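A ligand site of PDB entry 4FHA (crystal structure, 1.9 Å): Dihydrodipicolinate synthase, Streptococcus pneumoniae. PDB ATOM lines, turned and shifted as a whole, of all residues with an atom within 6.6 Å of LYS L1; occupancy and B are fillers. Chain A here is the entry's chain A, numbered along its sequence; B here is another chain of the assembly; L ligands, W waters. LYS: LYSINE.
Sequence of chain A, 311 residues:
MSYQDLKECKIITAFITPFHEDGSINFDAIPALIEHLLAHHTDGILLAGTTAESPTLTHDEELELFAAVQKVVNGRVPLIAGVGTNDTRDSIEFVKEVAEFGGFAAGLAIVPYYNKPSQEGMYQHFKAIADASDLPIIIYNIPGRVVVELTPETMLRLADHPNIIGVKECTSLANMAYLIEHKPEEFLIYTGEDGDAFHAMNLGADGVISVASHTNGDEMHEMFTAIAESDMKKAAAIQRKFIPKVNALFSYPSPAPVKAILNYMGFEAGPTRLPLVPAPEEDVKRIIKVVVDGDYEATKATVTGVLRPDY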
ATOM      1  N   ALA A  48     -17.590  24.972  -0.053  1.00  0.00           N
ATOM      2  CA  ALA A  48     -17.123  23.940  -1.003  1.00  0.00           C
ATOM      3  C   ALA A  48     -17.858  23.966  -2.347  1.00  0.00           C
ATOM      4  O   ALA A  48     -18.220  22.916  -2.888  1.00  0.00           O
ATOM      5  CB  ALA A  48     -17.152  22.554  -0.362  1.00  0.00           C
ATOM      6  N   GLU A  53     -12.894  26.290  -4.951  1.00  0.00           N
ATOM      7  CA  GLU A  53     -11.941  25.379  -5.601  1.00  0.00           C
ATOM      8  C   GLU A  53     -12.128  23.951  -5.083  1.00  0.00           C
ATOM      9  O   GLU A  53     -11.162  23.218  -4.850  1.00  0.00           O
ATOM     10  CB  GLU A  53     -10.487  25.836  -5.395  1.00  0.00           C
ATOM     11  CG  GLU A  53     -10.135  27.140  -6.092  1.00  0.00           C
ATOM     12  CD  GLU A  53      -8.779  27.678  -5.664  1.00  0.00           C
ATOM     13  OE1 GLU A  53      -8.753  28.635  -4.875  1.00  0.00           O
ATOM     14  OE2 GLU A  53      -7.753  27.139  -6.125  1.00  0.00           O
ATOM     15  N   SER A  54     -13.391  23.558  -4.908  1.00  0.00           N
ATOM     16  CA  SER A  54     -13.733  22.245  -4.371  1.00  0.00           C
ATOM     17  C   SER A  54     -13.140  21.062  -5.149  1.00  0.00           C
ATOM     18  O   SER A  54     -12.778  20.059  -4.524  1.00  0.00           O
ATOM     19  CB  SER A  54     -15.259  22.094  -4.214  1.00  0.00           C
ATOM     20  OG  SER A  54     -15.889  21.924  -5.467  1.00  0.00           O
ATOM     21  N   PRO A  55     -13.030  21.145  -6.497  1.00  0.00           N
ATOM     22  CA  PRO A  55     -12.438  20.002  -7.197  1.00  0.00           C
ATOM     23  C   PRO A  55     -10.981  19.697  -6.805  1.00  0.00           C
ATOM     24  O   PRO A  55     -10.495  18.603  -7.088  1.00  0.00           O
ATOM     25  CB  PRO A  55     -12.521  20.383  -8.677  1.00  0.00           C
ATOM     26  CG  PRO A  55     -12.843  21.832  -8.718  1.00  0.00           C
ATOM     27  CD  PRO A  55     -13.586  22.131  -7.445  1.00  0.00           C
ATOM     28  N   THR A  56     -10.307  20.659  -6.169  1.00  0.00           N
ATOM     29  CA  THR A  56      -8.929  20.445  -5.715  1.00  0.00           C
ATOM     30  C   THR A  56      -8.855  20.203  -4.205  1.00  0.00           C
ATOM     31  O   THR A  56      -7.774  20.049  -3.650  1.00  0.00           O
ATOM     32  CB  THR A  56      -7.993  21.614  -6.108  1.00  0.00           C
ATOM     33  OG1 THR A  56      -8.440  22.826  -5.492  1.00  0.00           O
ATOM     34  CG2 THR A  56      -7.937  21.789  -7.623  1.00  0.00           C
ATOM     35  N   LEU A  57     -10.013  20.169  -3.562  1.00  0.00           N
ATOM     36  CA  LEU A  57     -10.090  19.807  -2.149  1.00  0.00           C
ATOM     37  C   LEU A  57     -10.544  18.361  -1.996  1.00  0.00           C
ATOM     38  O   LEU A  57     -11.374  17.878  -2.761  1.00  0.00           O
ATOM     39  CB  LEU A  57     -11.078  20.719  -1.414  1.00  0.00           C
ATOM     40  CG  LEU A  57     -10.893  22.235  -1.461  1.00  0.00           C
ATOM     41  CD1 LEU A  57     -12.161  22.916  -0.957  1.00  0.00           C
ATOM     42  CD2 LEU A  57      -9.682  22.697  -0.655  1.00  0.00           C
ATOM     43  N   THR A  58      -9.973  17.661  -1.005  1.00  0.00           N
ATOM     44  CA  THR A  58     -10.446  16.328  -0.650  1.00  0.00           C
ATOM     45  C   THR A  58     -11.720  16.469   0.176  1.00  0.00           C
ATOM     46  O   THR A  58     -11.957  17.531   0.764  1.00  0.00           O
ATOM     47  CB  THR A  58      -9.410  15.559   0.185  1.00  0.00           C
ATOM     48  OG1 THR A  58      -9.163  16.257   1.412  1.00  0.00           O
ATOM     49  CG2 THR A  58      -8.100  15.394  -0.572  1.00  0.00           C
ATOM     50  N   HIS A  59     -12.518  15.415   0.217  1.00  0.00           N
ATOM     51  CA  HIS A  59     -13.724  15.383   1.065  1.00  0.00           C
ATOM     52  C   HIS A  59     -13.405  15.634   2.518  1.00  0.00           C
ATOM     53  O   HIS A  59     -14.156  16.312   3.215  1.00  0.00           O
ATOM     54  CB  HIS A  59     -14.482  14.077   0.897  1.00  0.00           C
ATOM     55  CG  HIS A  59     -15.340  14.017  -0.339  1.00  0.00           C
ATOM     56  ND1 HIS A  59     -16.172  15.019  -0.702  1.00  0.00           N
ATOM     57  CD2 HIS A  59     -15.496  13.020  -1.298  1.00  0.00           C
ATOM     58  CE1 HIS A  59     -16.814  14.685  -1.834  1.00  0.00           C
ATOM     59  NE2 HIS A  59     -16.404  13.454  -2.201  1.00  0.00           N
ATOM     60  N   GLU A  62     -12.765  19.311   3.079  1.00  0.00           N
ATOM     61  CA  GLU A  62     -14.039  20.018   3.073  1.00  0.00           C
ATOM     62  C   GLU A  62     -14.724  19.921   4.434  1.00  0.00           C
ATOM     63  O   GLU A  62     -15.258  20.917   4.930  1.00  0.00           O
ATOM     64  CB  GLU A  62     -14.919  19.517   1.936  1.00  0.00           C
ATOM     65  CG  GLU A  62     -14.390  19.899   0.561  1.00  0.00           C
ATOM     66  CD  GLU A  62     -15.091  19.201  -0.585  1.00  0.00           C
ATOM     67  OE1 GLU A  62     -15.696  18.136  -0.361  1.00  0.00           O
ATOM     68  OE2 GLU A  62     -15.012  19.705  -1.724  1.00  0.00           O
ATOM     69  N   GLY A  84     -21.913  17.441  -3.921  1.00  0.00           N
ATOM     70  CA  GLY A  84     -22.015  16.672  -5.162  1.00  0.00           C
ATOM     71  C   GLY A  84     -20.770  16.640  -6.030  1.00  0.00           C
ATOM     72  O   GLY A  84     -20.092  17.654  -6.209  1.00  0.00           O
ATOM     73  N   THR A  85     -20.459  15.458  -6.547  1.00  0.00           N
ATOM     74  CA  THR A  85     -19.431  15.318  -7.584  1.00  0.00           C
ATOM     75  C   THR A  85     -20.071  14.665  -8.805  1.00  0.00           C
ATOM     76  O   THR A  85     -21.294  14.478  -8.841  1.00  0.00           O
ATOM     77  CB  THR A  85     -18.222  14.486  -7.103  1.00  0.00           C
ATOM     78  OG1 THR A  85     -18.662  13.171  -6.714  1.00  0.00           O
ATOM     79  CG2 THR A  85     -17.519  15.163  -5.945  1.00  0.00           C
ATOM     80  N   ASN A  86     -19.262  14.328  -9.801  1.00  0.00           N
ATOM     81  CA  ASN A  86     -19.753  13.628 -10.995  1.00  0.00           C
ATOM     82  C   ASN A  86     -19.881  12.119 -10.808  1.00  0.00           C
ATOM     83  O   ASN A  86     -20.077  11.369 -11.770  1.00  0.00           O
ATOM     84  CB  ASN A  86     -18.870  13.942 -12.209  1.00  0.00           C
ATOM     85  CG  ASN A  86     -17.440  13.472 -12.043  1.00  0.00           C
ATOM     86  OD1 ASN A  86     -16.989  13.173 -10.937  1.00  0.00           O
ATOM     87  ND2 ASN A  86     -16.699  13.431 -13.152  1.00  0.00           N
ATOM     88  N   ASP A  87     -19.761  11.686  -9.551  1.00  0.00           N
ATOM     89  CA  ASP A  87     -19.825  10.284  -9.188  1.00  0.00           C
ATOM     90  C   ASP A  87     -20.934  10.121  -8.153  1.00  0.00           C
ATOM     91  O   ASP A  87     -20.805  10.573  -7.018  1.00  0.00           O
ATOM     92  CB  ASP A  87     -18.457   9.827  -8.638  1.00  0.00           C
ATOM     93  CG  ASP A  87     -18.452   8.371  -8.169  1.00  0.00           C
ATOM     94  OD1 ASP A  87     -19.433   7.635  -8.392  1.00  0.00           O
ATOM     95  OD2 ASP A  87     -17.439   7.971  -7.566  1.00  0.00           O
ATOM     96  N   ASP A  90     -19.969   8.407  -4.776  1.00  0.00           N
ATOM     97  CA  ASP A  90     -19.152   9.349  -4.015  1.00  0.00           C
ATOM     98  C   ASP A  90     -20.037  10.436  -3.378  1.00  0.00           C
ATOM     99  O   ASP A  90     -19.860  10.776  -2.217  1.00  0.00           O
ATOM    100  CB  ASP A  90     -18.098   9.991  -4.920  1.00  0.00           C
ATOM    101  CG  ASP A  90     -17.228  10.997  -4.165  1.00  0.00           C
ATOM    102  OD1 ASP A  90     -16.428  10.574  -3.300  1.00  0.00           O
ATOM    103  OD2 ASP A  90     -17.339  12.205  -4.450  1.00  0.00           O
ATOM    104  N   PHE A  94     -20.701  11.119   0.681  1.00  0.00           N
ATOM    105  CA  PHE A  94     -20.332  12.413   1.276  1.00  0.00           C
ATOM    106  C   PHE A  94     -21.517  13.153   1.891  1.00  0.00           C
ATOM    107  O   PHE A  94     -21.394  13.719   2.977  1.00  0.00           O
ATOM    108  CB  PHE A  94     -19.560  13.296   0.300  1.00  0.00           C
ATOM    109  CG  PHE A  94     -18.948  14.517   0.939  1.00  0.00           C
ATOM    110  CD1 PHE A  94     -17.985  14.373   1.952  1.00  0.00           C
ATOM    111  CD2 PHE A  94     -19.331  15.793   0.565  1.00  0.00           C
ATOM    112  CE1 PHE A  94     -17.415  15.490   2.550  1.00  0.00           C
ATOM    113  CE2 PHE A  94     -18.775  16.912   1.162  1.00  0.00           C
ATOM    114  CZ  PHE A  94     -17.817  16.761   2.154  1.00  0.00           C
ATOM    115  N   TYR A 113     -20.213  16.666 -14.234  1.00  0.00           N
ATOM    116  CA  TYR A 113     -19.282  17.184 -15.231  1.00  0.00           C
ATOM    117  C   TYR A 113     -18.482  16.065 -15.900  1.00  0.00           C
ATOM    118  O   TYR A 113     -18.360  14.969 -15.336  1.00  0.00           O
ATOM    119  CB  TYR A 113     -18.303  18.178 -14.580  1.00  0.00           C
ATOM    120  CG  TYR A 113     -17.907  17.794 -13.162  1.00  0.00           C
ATOM    121  CD1 TYR A 113     -18.637  18.247 -12.070  1.00  0.00           C
ATOM    122  CD2 TYR A 113     -16.810  16.958 -12.921  1.00  0.00           C
ATOM    123  CE1 TYR A 113     -18.296  17.886 -10.784  1.00  0.00           C
ATOM    124  CE2 TYR A 113     -16.455  16.595 -11.633  1.00  0.00           C
ATOM    125  CZ  TYR A 113     -17.216  17.058 -10.567  1.00  0.00           C
ATOM    126  OH  TYR A 113     -16.881  16.705  -9.282  1.00  0.00           O
ATOM    127  N   THR B  85      -6.805  13.662 -13.448  1.00  0.00           N
ATOM    128  CA  THR B  85      -8.113  14.220 -13.103  1.00  0.00           C
ATOM    129  C   THR B  85      -8.039  15.740 -13.219  1.00  0.00           C
ATOM    130  O   THR B  85      -7.086  16.275 -13.808  1.00  0.00           O
ATOM    131  CB  THR B  85      -8.565  13.830 -11.675  1.00  0.00           C
ATOM    132  OG1 THR B  85      -7.551  14.183 -10.720  1.00  0.00           O
ATOM    133  CG2 THR B  85      -8.858  12.331 -11.575  1.00  0.00           C
ATOM    134  N   ASN B  86      -9.027  16.449 -12.683  1.00  0.00           N
ATOM    135  CA  ASN B  86      -8.999  17.912 -12.650  1.00  0.00           C
ATOM    136  C   ASN B  86      -8.309  18.445 -11.392  1.00  0.00           C
ATOM    137  O   ASN B  86      -8.433  19.622 -11.048  1.00  0.00           O
ATOM    138  CB  ASN B  86     -10.412  18.488 -12.790  1.00  0.00           C
ATOM    139  CG  ASN B  86     -11.319  18.097 -11.625  1.00  0.00           C
ATOM    140  OD1 ASN B  86     -10.992  17.228 -10.813  1.00  0.00           O
ATOM    141  ND2 ASN B  86     -12.476  18.756 -11.548  1.00  0.00           N
ATOM    142  N   ASP B  87      -7.589  17.546 -10.709  1.00  0.00           N
ATOM    143  CA  ASP B  87      -6.856  17.851  -9.490  1.00  0.00           C
ATOM    144  C   ASP B  87      -5.406  17.457  -9.743  1.00  0.00           C
ATOM    145  O   ASP B  87      -5.081  16.271  -9.862  1.00  0.00           O
ATOM    146  CB  ASP B  87      -7.467  17.047  -8.332  1.00  0.00           C
ATOM    147  CG  ASP B  87      -6.792  17.309  -6.976  1.00  0.00           C
ATOM    148  OD1 ASP B  87      -5.623  17.746  -6.936  1.00  0.00           O
ATOM    149  OD2 ASP B  87      -7.436  17.039  -5.952  1.00  0.00           O
ATOM    150  N   ASP B  90      -3.807  15.087  -7.073  1.00  0.00           N
ATOM    151  CA  ASP B  90      -4.369  13.746  -7.280  1.00  0.00           C
ATOM    152  C   ASP B  90      -3.725  13.042  -8.479  1.00  0.00           C
ATOM    153  O   ASP B  90      -3.353  11.867  -8.399  1.00  0.00           O
ATOM    154  CB  ASP B  90      -5.886  13.806  -7.450  1.00  0.00           C
ATOM    155  CG  ASP B  90      -6.504  12.447  -7.725  1.00  0.00           C
ATOM    156  OD1 ASP B  90      -6.588  11.618  -6.797  1.00  0.00           O
ATOM    157  OD2 ASP B  90      -6.912  12.209  -8.888  1.00  0.00           O
ATOM    158  N   TYR B 113     -11.342  19.284 -16.126  1.00  0.00           N
ATOM    159  CA  TYR B 113     -12.772  19.551 -16.359  1.00  0.00           C
ATOM    160  C   TYR B 113     -13.357  20.331 -15.196  1.00  0.00           C
ATOM    161  O   TYR B 113     -12.833  20.280 -14.076  1.00  0.00           O
ATOM    162  CB  TYR B 113     -13.537  18.224 -16.547  1.00  0.00           C
ATOM    163  CG  TYR B 113     -13.006  17.102 -15.685  1.00  0.00           C
ATOM    164  CD1 TYR B 113     -11.964  16.296 -16.135  1.00  0.00           C
ATOM    165  CD2 TYR B 113     -13.541  16.858 -14.422  1.00  0.00           C
ATOM    166  CE1 TYR B 113     -11.472  15.268 -15.356  1.00  0.00           C
ATOM    167  CE2 TYR B 113     -13.045  15.823 -13.632  1.00  0.00           C
ATOM    168  CZ  TYR B 113     -12.004  15.038 -14.104  1.00  0.00           C
ATOM    169  OH  TYR B 113     -11.503  14.015 -13.335  1.00  0.00           O
ATOM    170  N   TYR B 114     -14.456  21.044 -15.469  1.00  0.00           N
ATOM    171  CA  TYR B 114     -15.233  21.763 -14.454  1.00  0.00           C
ATOM    172  C   TYR B 114     -14.578  23.083 -13.998  1.00  0.00           C
ATOM    173  O   TYR B 114     -15.213  24.137 -14.070  1.00  0.00           O
ATOM    174  CB  TYR B 114     -15.590  20.841 -13.268  1.00  0.00           C
ATOM    175  CG  TYR B 114     -16.351  21.472 -12.112  1.00  0.00           C
ATOM    176  CD1 TYR B 114     -17.246  22.519 -12.316  1.00  0.00           C
ATOM    177  CD2 TYR B 114     -16.193  20.987 -10.816  1.00  0.00           C
ATOM    178  CE1 TYR B 114     -17.933  23.100 -11.257  1.00  0.00           C
ATOM    179  CE2 TYR B 114     -16.891  21.548  -9.747  1.00  0.00           C
ATOM    180  CZ  TYR B 114     -17.760  22.597  -9.977  1.00  0.00           C
ATOM    181  OH  TYR B 114     -18.453  23.156  -8.938  1.00  0.00           O
ATOM    182  N   ASN B 115     -13.321  23.028 -13.564  1.00  0.00           N
ATOM    183  CA  ASN B 115     -12.647  24.234 -13.047  1.00  0.00           C
ATOM    184  C   ASN B 115     -12.119  25.197 -14.108  1.00  0.00           C
ATOM    185  O   ASN B 115     -11.688  26.298 -13.773  1.00  0.00           O
ATOM    186  CB  ASN B 115     -11.563  23.882 -12.011  1.00  0.00           C
ATOM    187  CG  ASN B 115     -10.680  22.721 -12.430  1.00  0.00           C
ATOM    188  OD1 ASN B 115     -10.608  22.374 -13.612  1.00  0.00           O
ATOM    189  ND2 ASN B 115     -10.006  22.121 -11.460  1.00  0.00           N
HETATM  190  N   LYS L   1     -11.318  16.324  -8.182  1.00  0.00           N
HETATM  191  CA  LYS L   1     -12.501  15.406  -8.151  1.00  0.00           C
HETATM  192  C   LYS L   1     -13.712  16.036  -8.821  1.00  0.00           C
HETATM  193  O   LYS L   1     -13.718  17.228  -9.139  1.00  0.00           O
HETATM  194  CB  LYS L   1     -12.830  14.986  -6.701  1.00  0.00           C
HETATM  195  CG  LYS L   1     -13.460  16.077  -5.852  1.00  0.00           C
HETATM  196  CD  LYS L   1     -13.532  15.652  -4.392  1.00  0.00           C
HETATM  197  CE  LYS L   1     -14.466  16.553  -3.598  1.00  0.00           C
HETATM  198  NZ  LYS L   1     -14.041  17.982  -3.591  1.00  0.00           N
HETATM  199  OXT LYS L   1     -14.711  15.359  -9.061  1.00  0.00           O
HETATM  200  N   LYS L   2     -15.098  11.237  -9.835  1.00  0.00           N
HETATM  201  CA  LYS L   2     -13.860  12.067  -9.741  1.00  0.00           C
HETATM  202  C   LYS L   2     -13.538  12.773 -11.059  1.00  0.00           C
HETATM  203  O   LYS L   2     -12.614  13.588 -11.135  1.00  0.00           O
HETATM  204  CB  LYS L   2     -12.659  11.214  -9.270  1.00  0.00           C
HETATM  205  CG  LYS L   2     -12.071  10.284 -10.309  1.00  0.00           C
HETATM  206  CD  LYS L   2     -11.069   9.322  -9.679  1.00  0.00           C
HETATM  207  CE  LYS L   2     -10.246   8.581 -10.726  1.00  0.00           C
HETATM  208  NZ  LYS L   2     -11.073   7.774 -11.671  1.00  0.00           N
HETATM  209  OXT LYS L   2     -14.200  12.548 -12.080  1.00  0.00           O
HETATM  210  O   HOH W   1      -9.360  14.285  -7.956  1.00  0.00           O
HETATM  211  O   HOH W   2     -15.842  18.826  -8.346  1.00  0.00           O
HETATM  212  O   HOH W   3     -10.181  16.362  -5.025  1.00  0.00           O
HETATM  213  O   HOH W   4     -15.633  19.042  -5.559  1.00  0.00           O
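CE1 of His 59 touches CE of LYS L1, 3.5 Å away.
OD1 of Asn 86 of chain A touches OXT of LYS L1, 3.7 Å away.
CB of Asp 87 of chain B touches N of LYS L1 (3.9 Å).
Water W4 bridges a nitrogen (NZ) of LYS L1 and the side-chain hydroxyl of Ser 54.
Water W2 bridges OH of Tyr 113 of chain A (2.5 Å) and O of LYS L1 (2.8 Å).
Water W1 lies within hydrogen-bond range of a nitrogen (N) of LYS L1, the side-chain hydroxyl of Thr 85 of chain B and the side-chain carboxylate of Asp 90 of chain B.
O of Pro 55 is in hydrogen-bond range of N of LYS L1 (2.7 Å).
The backbone carbonyl oxygen of Ser 54 lies within hydrogen-bond range of a nitrogen (NZ) of LYS L1.
OXT of LYS L1 lies within hydrogen-bond range of OH of Tyr 113 of chain A, at 2.6 Å.
The backbone carbonyl oxygen of Leu 57 lies within hydrogen-bond range of a nitrogen (NZ) of LYS L1.
The side-chain amide nitrogen of Asn 86 of chain A lies within hydrogen-bond range of an oxygen (OXT) of LYS L2 (2.9 Å).
A nitrogen (NZ) of LYS L1 is in salt-bridge range of the side-chain carboxylate (OE2) of Glu 62 (2.7 Å).
The side-chain hydroxyl (OH) of Tyr 113 of chain B sits at hydrogen-bond distance from an oxygen (O) of LYS L2, at 2.5 Å.
The side-chain amide oxygen of Asn 86 of chain B is in hydrogen-bond range of a nitrogen (N) of LYS L1 (2.8 Å).
The side-chain hydroxyl (OG1) of Thr 85 of chain B is in hydrogen-bond range of the backbone carbonyl oxygen (O) of Asp 87 of chain B.
A ring nitrogen (NE2) of His 59 sits at hydrogen-bond distance from the side-chain carboxylate of Asp 90 of chain A (2.7 Å).
The backbone carbonyl oxygen (O) of Tyr 113 of chain A is in hydrogen-bond range of the side-chain amide nitrogen (ND2) of Asn 86 of chain A (3.1 Å).
The side-chain carboxylate (OD1) of Asp 87 of chain B sits at hydrogen-bond distance from the backbone NH (N) of Asp 90 of chain B, at 3.2 Å.
The backbone carbonyl oxygen of Tyr 113 of chain B is in hydrogen-bond range of the side-chain amide nitrogen of Asn 86 of chain B, at 3.0 Å.
ND1 of His 59 lies within hydrogen-bond range of OE1 of Glu 62, 3.2 Å away.
ND2 of Asn 115 of chain B is in hydrogen-bond range of O of Asn 86 of chain B (3.0 Å).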
